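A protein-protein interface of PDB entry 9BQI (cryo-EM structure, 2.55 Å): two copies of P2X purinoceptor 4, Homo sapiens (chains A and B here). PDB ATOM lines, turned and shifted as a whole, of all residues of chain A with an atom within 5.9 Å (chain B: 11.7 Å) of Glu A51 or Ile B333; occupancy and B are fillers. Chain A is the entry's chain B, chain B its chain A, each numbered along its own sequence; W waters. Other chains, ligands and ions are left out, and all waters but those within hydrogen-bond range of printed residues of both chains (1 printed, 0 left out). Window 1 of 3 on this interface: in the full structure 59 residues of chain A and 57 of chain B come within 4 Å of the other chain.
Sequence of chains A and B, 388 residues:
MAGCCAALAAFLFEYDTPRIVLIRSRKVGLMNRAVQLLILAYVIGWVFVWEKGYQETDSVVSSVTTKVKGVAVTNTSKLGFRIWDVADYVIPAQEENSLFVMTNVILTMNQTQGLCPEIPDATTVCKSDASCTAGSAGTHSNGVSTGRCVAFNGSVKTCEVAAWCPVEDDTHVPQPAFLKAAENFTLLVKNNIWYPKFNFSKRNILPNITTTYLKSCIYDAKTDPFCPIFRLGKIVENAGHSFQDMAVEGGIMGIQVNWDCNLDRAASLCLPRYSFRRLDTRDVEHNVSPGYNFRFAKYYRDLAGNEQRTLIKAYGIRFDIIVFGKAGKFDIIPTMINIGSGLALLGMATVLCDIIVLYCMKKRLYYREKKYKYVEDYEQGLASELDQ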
ATOM      1  N   TYR A  42      25.615 -15.702  -8.778  1.00  0.00           N
ATOM      2  CA  TYR A  42      26.179 -15.634  -7.437  1.00  0.00           C
ATOM      3  C   TYR A  42      25.148 -16.068  -6.403  1.00  0.00           C
ATOM      4  O   TYR A  42      25.321 -17.081  -5.716  1.00  0.00           O
ATOM      5  CB  TYR A  42      26.673 -14.216  -7.143  1.00  0.00           C
ATOM      6  CG  TYR A  42      26.965 -13.975  -5.681  1.00  0.00           C
ATOM      7  CD1 TYR A  42      28.079 -14.536  -5.072  1.00  0.00           C
ATOM      8  CD2 TYR A  42      26.124 -13.191  -4.905  1.00  0.00           C
ATOM      9  CE1 TYR A  42      28.346 -14.325  -3.735  1.00  0.00           C
ATOM     10  CE2 TYR A  42      26.382 -12.972  -3.566  1.00  0.00           C
ATOM     11  CZ  TYR A  42      27.495 -13.543  -2.988  1.00  0.00           C
ATOM     12  OH  TYR A  42      27.757 -13.329  -1.656  1.00  0.00           O
ATOM     13  N   GLY A  45      23.939 -20.005  -7.017  1.00  0.00           N
ATOM     14  CA  GLY A  45      24.957 -21.035  -6.910  1.00  0.00           C
ATOM     15  C   GLY A  45      25.776 -20.930  -5.640  1.00  0.00           C
ATOM     16  O   GLY A  45      25.836 -21.873  -4.847  1.00  0.00           O
ATOM     17  N   TRP A  46      26.420 -19.781  -5.425  1.00  0.00           N
ATOM     18  CA  TRP A  46      27.385 -19.697  -4.337  1.00  0.00           C
ATOM     19  C   TRP A  46      26.699 -19.668  -2.977  1.00  0.00           C
ATOM     20  O   TRP A  46      27.150 -20.333  -2.040  1.00  0.00           O
ATOM     21  CB  TRP A  46      28.268 -18.465  -4.515  1.00  0.00           C
ATOM     22  CG  TRP A  46      29.482 -18.490  -3.644  1.00  0.00           C
ATOM     23  CD1 TRP A  46      29.728 -17.708  -2.555  1.00  0.00           C
ATOM     24  CD2 TRP A  46      30.616 -19.353  -3.783  1.00  0.00           C
ATOM     25  NE1 TRP A  46      30.946 -18.026  -2.010  1.00  0.00           N
ATOM     26  CE2 TRP A  46      31.511 -19.035  -2.745  1.00  0.00           C
ATOM     27  CE3 TRP A  46      30.960 -20.364  -4.684  1.00  0.00           C
ATOM     28  CZ2 TRP A  46      32.729 -19.690  -2.584  1.00  0.00           C
ATOM     29  CZ3 TRP A  46      32.169 -21.012  -4.524  1.00  0.00           C
ATOM     30  CH2 TRP A  46      33.040 -20.673  -3.483  1.00  0.00           C
ATOM     31  N   VAL A  47      25.608 -18.914  -2.850  1.00  0.00           N
ATOM     32  CA  VAL A  47      24.989 -18.728  -1.544  1.00  0.00           C
ATOM     33  C   VAL A  47      24.073 -19.897  -1.205  1.00  0.00           C
ATOM     34  O   VAL A  47      24.135 -20.446  -0.100  1.00  0.00           O
ATOM     35  CB  VAL A  47      24.239 -17.385  -1.497  1.00  0.00           C
ATOM     36  CG1 VAL A  47      23.477 -17.242  -0.190  1.00  0.00           C
ATOM     37  CG2 VAL A  47      25.206 -16.232  -1.681  1.00  0.00           C
ATOM     38  N   PHE A  48      23.208 -20.298  -2.140  1.00  0.00           N
ATOM     39  CA  PHE A  48      22.213 -21.324  -1.847  1.00  0.00           C
ATOM     40  C   PHE A  48      22.736 -22.723  -2.167  1.00  0.00           C
ATOM     41  O   PHE A  48      22.799 -23.587  -1.287  1.00  0.00           O
ATOM     42  CB  PHE A  48      20.926 -21.043  -2.630  1.00  0.00           C
ATOM     43  CG  PHE A  48      20.056 -19.982  -2.014  1.00  0.00           C
ATOM     44  CD1 PHE A  48      19.678 -20.054  -0.685  1.00  0.00           C
ATOM     45  CD2 PHE A  48      19.612 -18.911  -2.771  1.00  0.00           C
ATOM     46  CE1 PHE A  48      18.882 -19.080  -0.123  1.00  0.00           C
ATOM     47  CE2 PHE A  48      18.815 -17.935  -2.214  1.00  0.00           C
ATOM     48  CZ  PHE A  48      18.450 -18.021  -0.888  1.00  0.00           C
ATOM     49  N   VAL A  49      23.114 -22.960  -3.425  1.00  0.00           N
ATOM     50  CA  VAL A  49      23.482 -24.309  -3.847  1.00  0.00           C
ATOM     51  C   VAL A  49      24.811 -24.723  -3.227  1.00  0.00           C
ATOM     52  O   VAL A  49      24.954 -25.842  -2.720  1.00  0.00           O
ATOM     53  CB  VAL A  49      23.527 -24.392  -5.383  1.00  0.00           C
ATOM     54  CG1 VAL A  49      24.209 -25.675  -5.826  1.00  0.00           C
ATOM     55  CG2 VAL A  49      22.124 -24.300  -5.961  1.00  0.00           C
ATOM     56  N   TRP A  50      25.802 -23.835  -3.258  1.00  0.00           N
ATOM     57  CA  TRP A  50      27.157 -24.193  -2.851  1.00  0.00           C
ATOM     58  C   TRP A  50      27.369 -24.054  -1.348  1.00  0.00           C
ATOM     59  O   TRP A  50      27.777 -25.013  -0.685  1.00  0.00           O
ATOM     60  CB  TRP A  50      28.174 -23.333  -3.604  1.00  0.00           C
ATOM     61  CG  TRP A  50      29.589 -23.782  -3.415  1.00  0.00           C
ATOM     62  CD1 TRP A  50      30.485 -23.307  -2.503  1.00  0.00           C
ATOM     63  CD2 TRP A  50      30.275 -24.796  -4.159  1.00  0.00           C
ATOM     64  NE1 TRP A  50      31.684 -23.962  -2.630  1.00  0.00           N
ATOM     65  CE2 TRP A  50      31.582 -24.881  -3.642  1.00  0.00           C
ATOM     66  CE3 TRP A  50      29.911 -25.640  -5.213  1.00  0.00           C
ATOM     67  CZ2 TRP A  50      32.526 -25.776  -4.140  1.00  0.00           C
ATOM     68  CZ3 TRP A  50      30.850 -26.528  -5.706  1.00  0.00           C
ATOM     69  CH2 TRP A  50      32.140 -26.589  -5.171  1.00  0.00           C
ATOM     70  N   GLU A  51      27.102 -22.874  -0.795  1.00  0.00           N
ATOM     71  CA  GLU A  51      27.387 -22.591   0.606  1.00  0.00           C
ATOM     72  C   GLU A  51      26.215 -22.890   1.530  1.00  0.00           C
ATOM     73  O   GLU A  51      26.333 -22.667   2.740  1.00  0.00           O
ATOM     74  CB  GLU A  51      27.808 -21.129   0.770  1.00  0.00           C
ATOM     75  CG  GLU A  51      29.069 -20.762   0.005  1.00  0.00           C
ATOM     76  CD  GLU A  51      30.331 -21.042   0.793  1.00  0.00           C
ATOM     77  OE1 GLU A  51      30.377 -20.702   1.993  1.00  0.00           O
ATOM     78  OE2 GLU A  51      31.282 -21.602   0.207  1.00  0.00           O
ATOM     79  N   LYS A  52      25.099 -23.386   1.002  1.00  0.00           N
ATOM     80  CA  LYS A  52      23.939 -23.752   1.812  1.00  0.00           C
ATOM     81  C   LYS A  52      23.495 -22.579   2.687  1.00  0.00           C
ATOM     82  O   LYS A  52      23.508 -22.638   3.916  1.00  0.00           O
ATOM     83  CB  LYS A  52      24.246 -24.984   2.664  1.00  0.00           C
ATOM     84  CG  LYS A  52      24.615 -26.226   1.868  1.00  0.00           C
ATOM     85  CD  LYS A  52      23.452 -26.723   1.033  1.00  0.00           C
ATOM     86  CE  LYS A  52      23.772 -28.052   0.372  1.00  0.00           C
ATOM     87  NZ  LYS A  52      24.807 -27.910  -0.686  1.00  0.00           N
ATOM     88  N   GLY A  53      23.091 -21.502   2.019  1.00  0.00           N
ATOM     89  CA  GLY A  53      22.644 -20.297   2.685  1.00  0.00           C
ATOM     90  C   GLY A  53      21.218 -20.333   3.174  1.00  0.00           C
ATOM     91  O   GLY A  53      20.725 -19.332   3.697  1.00  0.00           O
ATOM     92  N   ASN A 338      18.713 -13.868   2.429  1.00  0.00           N
ATOM     93  CA  ASN A 338      19.477 -13.953   1.190  1.00  0.00           C
ATOM     94  C   ASN A 338      18.660 -13.463   0.001  1.00  0.00           C
ATOM     95  O   ASN A 338      19.188 -12.782  -0.887  1.00  0.00           O
ATOM     96  CB  ASN A 338      19.942 -15.390   0.969  1.00  0.00           C
ATOM     97  CG  ASN A 338      20.974 -15.831   1.987  1.00  0.00           C
ATOM     98  OD1 ASN A 338      20.781 -16.814   2.699  1.00  0.00           O
ATOM     99  ND2 ASN A 338      22.081 -15.107   2.058  1.00  0.00           N
ATOM    100  N   VAL B  47      29.717  -1.320  10.908  1.00  0.00           N
ATOM    101  CA  VAL B  47      29.533  -2.698  10.465  1.00  0.00           C
ATOM    102  C   VAL B  47      30.832  -3.266   9.905  1.00  0.00           C
ATOM    103  O   VAL B  47      31.235  -4.379  10.258  1.00  0.00           O
ATOM    104  CB  VAL B  47      28.390  -2.778   9.438  1.00  0.00           C
ATOM    105  CG1 VAL B  47      28.280  -4.183   8.868  1.00  0.00           C
ATOM    106  CG2 VAL B  47      27.078  -2.355  10.072  1.00  0.00           C
ATOM    107  N   PHE B  48      31.507  -2.522   9.028  1.00  0.00           N
ATOM    108  CA  PHE B  48      32.690  -3.048   8.356  1.00  0.00           C
ATOM    109  C   PHE B  48      33.968  -2.741   9.135  1.00  0.00           C
ATOM    110  O   PHE B  48      34.698  -3.655   9.527  1.00  0.00           O
ATOM    111  CB  PHE B  48      32.781  -2.476   6.936  1.00  0.00           C
ATOM    112  CG  PHE B  48      31.876  -3.156   5.945  1.00  0.00           C
ATOM    113  CD1 PHE B  48      31.887  -4.531   5.797  1.00  0.00           C
ATOM    114  CD2 PHE B  48      31.014  -2.413   5.156  1.00  0.00           C
ATOM    115  CE1 PHE B  48      31.058  -5.152   4.888  1.00  0.00           C
ATOM    116  CE2 PHE B  48      30.181  -3.029   4.246  1.00  0.00           C
ATOM    117  CZ  PHE B  48      30.205  -4.401   4.113  1.00  0.00           C
ATOM    118  N   LYS B  52      33.760  -5.503  12.032  1.00  0.00           N
ATOM    119  CA  LYS B  52      34.283  -6.521  11.123  1.00  0.00           C
ATOM    120  C   LYS B  52      33.150  -7.375  10.554  1.00  0.00           C
ATOM    121  O   LYS B  52      33.073  -8.586  10.764  1.00  0.00           O
ATOM    122  CB  LYS B  52      35.322  -7.392  11.832  1.00  0.00           C
ATOM    123  CG  LYS B  52      36.529  -6.632  12.356  1.00  0.00           C
ATOM    124  CD  LYS B  52      37.353  -6.042  11.229  1.00  0.00           C
ATOM    125  CE  LYS B  52      38.643  -5.429  11.746  1.00  0.00           C
ATOM    126  NZ  LYS B  52      38.391  -4.205  12.552  1.00  0.00           N
ATOM    127  N   GLY B  53      32.262  -6.713   9.815  1.00  0.00           N
ATOM    128  CA  GLY B  53      31.121  -7.360   9.206  1.00  0.00           C
ATOM    129  C   GLY B  53      31.416  -8.086   7.916  1.00  0.00           C
ATOM    130  O   GLY B  53      30.497  -8.613   7.287  1.00  0.00           O
ATOM    131  N   TYR B  54      32.681  -8.121   7.501  1.00  0.00           N
ATOM    132  CA  TYR B  54      33.104  -8.762   6.264  1.00  0.00           C
ATOM    133  C   TYR B  54      33.803 -10.092   6.509  1.00  0.00           C
ATOM    134  O   TYR B  54      34.521 -10.575   5.627  1.00  0.00           O
ATOM    135  CB  TYR B  54      34.029  -7.825   5.487  1.00  0.00           C
ATOM    136  CG  TYR B  54      35.261  -7.417   6.266  1.00  0.00           C
ATOM    137  CD1 TYR B  54      36.414  -8.189   6.234  1.00  0.00           C
ATOM    138  CD2 TYR B  54      35.267  -6.267   7.040  1.00  0.00           C
ATOM    139  CE1 TYR B  54      37.536  -7.825   6.947  1.00  0.00           C
ATOM    140  CE2 TYR B  54      36.384  -5.895   7.755  1.00  0.00           C
ATOM    141  CZ  TYR B  54      37.516  -6.677   7.706  1.00  0.00           C
ATOM    142  OH  TYR B  54      38.631  -6.307   8.420  1.00  0.00           O
ATOM    143  N   GLN B  55      33.611 -10.695   7.680  1.00  0.00           N
ATOM    144  CA  GLN B  55      34.406 -11.833   8.108  1.00  0.00           C
ATOM    145  C   GLN B  55      33.516 -12.993   8.526  1.00  0.00           C
ATOM    146  O   GLN B  55      32.397 -12.801   9.004  1.00  0.00           O
ATOM    147  CB  GLN B  55      35.319 -11.454   9.278  1.00  0.00           C
ATOM    148  CG  GLN B  55      36.470 -10.553   8.891  1.00  0.00           C
ATOM    149  CD  GLN B  55      37.528 -10.478   9.962  1.00  0.00           C
ATOM    150  OE1 GLN B  55      37.240 -10.624  11.148  1.00  0.00           O
ATOM    151  NE2 GLN B  55      38.768 -10.257   9.551  1.00  0.00           N
ATOM    152  N   GLU B  56      34.038 -14.202   8.335  1.00  0.00           N
ATOM    153  CA  GLU B  56      33.456 -15.420   8.877  1.00  0.00           C
ATOM    154  C   GLU B  56      34.247 -15.855  10.104  1.00  0.00           C
ATOM    155  O   GLU B  56      35.473 -15.727  10.151  1.00  0.00           O
ATOM    156  CB  GLU B  56      33.448 -16.535   7.829  1.00  0.00           C
ATOM    157  CG  GLU B  56      34.833 -17.005   7.407  1.00  0.00           C
ATOM    158  CD  GLU B  56      34.785 -18.063   6.322  1.00  0.00           C
ATOM    159  OE1 GLU B  56      33.671 -18.416   5.883  1.00  0.00           O
ATOM    160  OE2 GLU B  56      35.862 -18.537   5.907  1.00  0.00           O
ATOM    161  N   THR B  57      33.535 -16.371  11.102  1.00  0.00           N
ATOM    162  CA  THR B  57      34.112 -16.673  12.405  1.00  0.00           C
ATOM    163  C   THR B  57      34.121 -18.173  12.656  1.00  0.00           C
ATOM    164  O   THR B  57      33.199 -18.887  12.252  1.00  0.00           O
ATOM    165  CB  THR B  57      33.338 -15.969  13.525  1.00  0.00           C
ATOM    166  OG1 THR B  57      31.982 -16.432  13.538  1.00  0.00           O
ATOM    167  CG2 THR B  57      33.356 -14.461  13.321  1.00  0.00           C
ATOM    168  N   LYS B 197      38.097 -24.780  10.522  1.00  0.00           N
ATOM    169  CA  LYS B 197      37.533 -24.129   9.343  1.00  0.00           C
ATOM    170  C   LYS B 197      38.625 -23.536   8.462  1.00  0.00           C
ATOM    171  O   LYS B 197      38.592 -23.688   7.235  1.00  0.00           O
ATOM    172  CB  LYS B 197      36.548 -23.042   9.769  1.00  0.00           C
ATOM    173  CG  LYS B 197      35.797 -22.391   8.620  1.00  0.00           C
ATOM    174  CD  LYS B 197      34.895 -21.269   9.110  1.00  0.00           C
ATOM    175  CE  LYS B 197      33.671 -21.806   9.825  1.00  0.00           C
ATOM    176  NZ  LYS B 197      32.716 -20.725  10.190  1.00  0.00           N
ATOM    177  N   PHE B 198      39.597 -22.857   9.065  1.00  0.00           N
ATOM    178  CA  PHE B 198      40.655 -22.180   8.329  1.00  0.00           C
ATOM    179  C   PHE B 198      41.937 -22.994   8.231  1.00  0.00           C
ATOM    180  O   PHE B 198      42.903 -22.526   7.620  1.00  0.00           O
ATOM    181  CB  PHE B 198      40.963 -20.828   8.978  1.00  0.00           C
ATOM    182  CG  PHE B 198      39.743 -20.011   9.295  1.00  0.00           C
ATOM    183  CD1 PHE B 198      38.910 -19.563   8.286  1.00  0.00           C
ATOM    184  CD2 PHE B 198      39.434 -19.686  10.604  1.00  0.00           C
ATOM    185  CE1 PHE B 198      37.789 -18.809   8.578  1.00  0.00           C
ATOM    186  CE2 PHE B 198      38.315 -18.934  10.898  1.00  0.00           C
ATOM    187  CZ  PHE B 198      37.493 -18.496   9.885  1.00  0.00           C
ATOM    188  N   LYS B 329      38.216 -14.460   9.269  1.00  0.00           N
ATOM    189  CA  LYS B 329      38.800 -14.338   7.942  1.00  0.00           C
ATOM    190  C   LYS B 329      37.764 -13.729   7.012  1.00  0.00           C
ATOM    191  O   LYS B 329      36.560 -13.928   7.185  1.00  0.00           O
ATOM    192  CB  LYS B 329      39.264 -15.700   7.407  1.00  0.00           C
ATOM    193  CG  LYS B 329      40.625 -15.676   6.739  1.00  0.00           C
ATOM    194  CD  LYS B 329      41.106 -17.083   6.429  1.00  0.00           C
ATOM    195  CE  LYS B 329      42.571 -17.100   6.020  1.00  0.00           C
ATOM    196  NZ  LYS B 329      42.842 -16.210   4.859  1.00  0.00           N
ATOM    197  N   PHE B 330      38.242 -12.981   6.021  1.00  0.00           N
ATOM    198  CA  PHE B 330      37.340 -12.313   5.094  1.00  0.00           C
ATOM    199  C   PHE B 330      36.488 -13.330   4.346  1.00  0.00           C
ATOM    200  O   PHE B 330      36.988 -14.352   3.872  1.00  0.00           O
ATOM    201  CB  PHE B 330      38.134 -11.462   4.103  1.00  0.00           C
ATOM    202  CG  PHE B 330      37.336 -11.021   2.910  1.00  0.00           C
ATOM    203  CD1 PHE B 330      36.517  -9.907   2.983  1.00  0.00           C
ATOM    204  CD2 PHE B 330      37.402 -11.719   1.718  1.00  0.00           C
ATOM    205  CE1 PHE B 330      35.781  -9.501   1.890  1.00  0.00           C
ATOM    206  CE2 PHE B 330      36.665 -11.318   0.622  1.00  0.00           C
ATOM    207  CZ  PHE B 330      35.855 -10.208   0.708  1.00  0.00           C
ATOM    208  N   ASP B 331      35.190 -13.043   4.246  1.00  0.00           N
ATOM    209  CA  ASP B 331      34.258 -13.867   3.492  1.00  0.00           C
ATOM    210  C   ASP B 331      33.346 -12.956   2.684  1.00  0.00           C
ATOM    211  O   ASP B 331      33.036 -11.838   3.100  1.00  0.00           O
ATOM    212  CB  ASP B 331      33.429 -14.773   4.412  1.00  0.00           C
ATOM    213  CG  ASP B 331      32.849 -15.973   3.687  1.00  0.00           C
ATOM    214  OD1 ASP B 331      33.232 -16.213   2.523  1.00  0.00           O
ATOM    215  OD2 ASP B 331      32.010 -16.679   4.283  1.00  0.00           O
ATOM    216  N   ILE B 332      32.916 -13.448   1.521  1.00  0.00           N
ATOM    217  CA  ILE B 332      32.159 -12.605   0.600  1.00  0.00           C
ATOM    218  C   ILE B 332      30.671 -12.595   0.941  1.00  0.00           C
ATOM    219  O   ILE B 332      29.968 -11.628   0.624  1.00  0.00           O
ATOM    220  CB  ILE B 332      32.397 -13.069  -0.849  1.00  0.00           C
ATOM    221  CG1 ILE B 332      31.857 -12.040  -1.847  1.00  0.00           C
ATOM    222  CG2 ILE B 332      31.747 -14.423  -1.093  1.00  0.00           C
ATOM    223  CD1 ILE B 332      32.613 -10.731  -1.854  1.00  0.00           C
ATOM    224  N   ILE B 333      30.164 -13.644   1.581  1.00  0.00           N
ATOM    225  CA  ILE B 333      28.735 -13.749   1.871  1.00  0.00           C
ATOM    226  C   ILE B 333      28.308 -12.634   2.823  1.00  0.00           C
ATOM    227  O   ILE B 333      27.381 -11.877   2.495  1.00  0.00           O
ATOM    228  CB  ILE B 333      28.386 -15.135   2.439  1.00  0.00           C
ATOM    229  CG1 ILE B 333      28.626 -16.213   1.381  1.00  0.00           C
ATOM    230  CG2 ILE B 333      26.939 -15.172   2.910  1.00  0.00           C
ATOM    231  CD1 ILE B 333      28.569 -17.620   1.921  1.00  0.00           C
ATOM    232  N   PRO B 334      28.921 -12.497   4.003  1.00  0.00           N
ATOM    233  CA  PRO B 334      28.541 -11.380   4.883  1.00  0.00           C
ATOM    234  C   PRO B 334      28.782 -10.017   4.264  1.00  0.00           C
ATOM    235  O   PRO B 334      27.999  -9.090   4.503  1.00  0.00           O
ATOM    236  CB  PRO B 334      29.412 -11.602   6.130  1.00  0.00           C
ATOM    237  CG  PRO B 334      30.512 -12.498   5.689  1.00  0.00           C
ATOM    238  CD  PRO B 334      29.923 -13.370   4.637  1.00  0.00           C
ATOM    239  N   THR B 335      29.843  -9.868   3.471  1.00  0.00           N
ATOM    240  CA  THR B 335      30.102  -8.595   2.805  1.00  0.00           C
ATOM    241  C   THR B 335      28.940  -8.214   1.897  1.00  0.00           C
ATOM    242  O   THR B 335      28.424  -7.091   1.958  1.00  0.00           O
ATOM    243  CB  THR B 335      31.400  -8.684   2.003  1.00  0.00           C
ATOM    244  OG1 THR B 335      32.458  -9.145   2.851  1.00  0.00           O
ATOM    245  CG2 THR B 335      31.773  -7.330   1.425  1.00  0.00           C
ATOM    246  N   MET B 336      28.511  -9.149   1.048  1.00  0.00           N
ATOM    247  CA  MET B 336      27.410  -8.874   0.133  1.00  0.00           C
ATOM    248  C   MET B 336      26.106  -8.663   0.892  1.00  0.00           C
ATOM    249  O   MET B 336      25.285  -7.828   0.498  1.00  0.00           O
ATOM    250  CB  MET B 336      27.276 -10.014  -0.871  1.00  0.00           C
ATOM    251  CG  MET B 336      28.451 -10.136  -1.831  1.00  0.00           C
ATOM    252  SD  MET B 336      28.288  -9.109  -3.302  1.00  0.00           S
ATOM    253  CE  MET B 336      29.373  -7.752  -2.885  1.00  0.00           C
ATOM    254  N   ILE B 337      25.899  -9.403   1.982  1.00  0.00           N
ATOM    255  CA  ILE B 337      24.694  -9.214   2.788  1.00  0.00           C
ATOM    256  C   ILE B 337      24.648  -7.796   3.340  1.00  0.00           C
ATOM    257  O   ILE B 337      23.619  -7.114   3.271  1.00  0.00           O
ATOM    258  CB  ILE B 337      24.634 -10.259   3.917  1.00  0.00           C
ATOM    259  CG1 ILE B 337      24.475 -11.667   3.339  1.00  0.00           C
ATOM    260  CG2 ILE B 337      23.498  -9.940   4.879  1.00  0.00           C
ATOM    261  CD1 ILE B 337      23.053 -12.039   3.004  1.00  0.00           C
ATOM    262  N   ASN B 338      25.768  -7.330   3.896  1.00  0.00           N
ATOM    263  CA  ASN B 338      25.815  -5.989   4.465  1.00  0.00           C
ATOM    264  C   ASN B 338      25.644  -4.925   3.389  1.00  0.00           C
ATOM    265  O   ASN B 338      24.961  -3.915   3.607  1.00  0.00           O
ATOM    266  CB  ASN B 338      27.131  -5.792   5.214  1.00  0.00           C
ATOM    267  CG  ASN B 338      27.226  -6.649   6.459  1.00  0.00           C
ATOM    268  OD1 ASN B 338      28.148  -7.449   6.608  1.00  0.00           O
ATOM    269  ND2 ASN B 338      26.275  -6.482   7.366  1.00  0.00           N
ATOM    270  N   ILE B 339      26.252  -5.131   2.219  1.00  0.00           N
ATOM    271  CA  ILE B 339      26.121  -4.163   1.133  1.00  0.00           C
ATOM    272  C   ILE B 339      24.668  -4.069   0.676  1.00  0.00           C
ATOM    273  O   ILE B 339      24.129  -2.972   0.477  1.00  0.00           O
ATOM    274  CB  ILE B 339      27.063  -4.535  -0.025  1.00  0.00           C
ATOM    275  CG1 ILE B 339      28.514  -4.272   0.389  1.00  0.00           C
ATOM    276  CG2 ILE B 339      26.701  -3.747  -1.280  1.00  0.00           C
ATOM    277  CD1 ILE B 339      29.549  -4.811  -0.572  1.00  0.00           C
ATOM    278  N   GLY B 340      24.012  -5.219   0.504  1.00  0.00           N
ATOM    279  CA  GLY B 340      22.611  -5.207   0.113  1.00  0.00           C
ATOM    280  C   GLY B 340      21.719  -4.569   1.159  1.00  0.00           C
ATOM    281  O   GLY B 340      20.786  -3.831   0.831  1.00  0.00           O
ATOM    282  N   SER B 341      21.987  -4.850   2.436  1.00  0.00           N
ATOM    283  CA  SER B 341      21.202  -4.239   3.503  1.00  0.00           C
ATOM    284  C   SER B 341      21.365  -2.724   3.510  1.00  0.00           C
ATOM    285  O   SER B 341      20.391  -1.992   3.704  1.00  0.00           O
ATOM    286  CB  SER B 341      21.607  -4.829   4.852  1.00  0.00           C
ATOM    287  OG  SER B 341      20.853  -4.254   5.904  1.00  0.00           O
ATOM    288  N   GLY B 342      22.591  -2.235   3.309  1.00  0.00           N
ATOM    289  CA  GLY B 342      22.793  -0.797   3.218  1.00  0.00           C
ATOM    290  C   GLY B 342      22.084  -0.185   2.024  1.00  0.00           C
ATOM    291  O   GLY B 342      21.494   0.897   2.122  1.00  0.00           O
HETATM  292  O   HOH W   1      26.021 -12.773   0.420  1.00  0.00           O
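Among the printed residues, merely in contact across the chains: Tyr A42 with Met B336, Asn A338 with Ile B337, Glu A51 with Ile B333, Tyr A42 with Ile B332, Tyr A42 with Ile B333 and Trp A46 with Ile B332.
The backbone NH (N) of Glu A51 lies within hydrogen-bond range of the backbone carbonyl oxygen (O) of Trp A46, at 2.8 Å. The backbone carbonyl oxygen of Gly A53 lies close to the side-chain amide oxygen of Asn A338, 2.7 Å away. O of Tyr A42 is in hydrogen-bond range of N of Val A47, at 3.4 Å.
Water W1 lies within hydrogen-bond range of O of Ile B333 (2.6 Å) and OH of Tyr A42 (2.8 Å).
Of the 24 printed residues of chain B, 4 touch a printed residue of chain A. Hydrophobic or aromatic side chains of chain A that line the printed part of chain B: Tyr A42 and Trp A46. Along chain A the printed residues that touch a printed residue of chain B span positions 42 to 338. Among the printed residues, no Asp or Glu carboxylate lies within 4 Å of a Lys or Arg side-chain nitrogen of the other chain.
5 positions are printed for both chains.
Of the printed residues of chain B, Glu A51 touches Ile B333 (3.6 Å). Of chain A, only Tyr A42 (3.7 Å) and Glu A51 (3.6 Å) come within 4 Å of Ile B333. Trp A46 touches one residue of chain B. No residue of chain B comes within 4 Å of Val A47. No residue of chain B comes within 4 Å of Val A49. Trp A50 touches none of the printed residues of chain B. Gly A53 touches none of the printed residues of chain B. Of the printed residues of chain A, Met B336 touches Tyr A42 (3.3 Å). Of the printed residues of chain B, Tyr A42 touches Ile B332 (3.6 Å), Ile B333 (3.7 Å) and Met B336 (3.3 Å). Of the printed residues of chain A, Ile B332 touches Tyr A42 and Trp A46. Printed residues of chain A within 4 Å of Ile B337: Asn A338. Printed residues of chain B within 4 Å of Asn A338: Ile B337. Lys B329 touches none of the printed residues of chain A. Lys B52 touches none of the printed residues of chain A. The nearest printed residue of chain B that does not touch Asn A338 is Ile B333 (4.9 Å).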
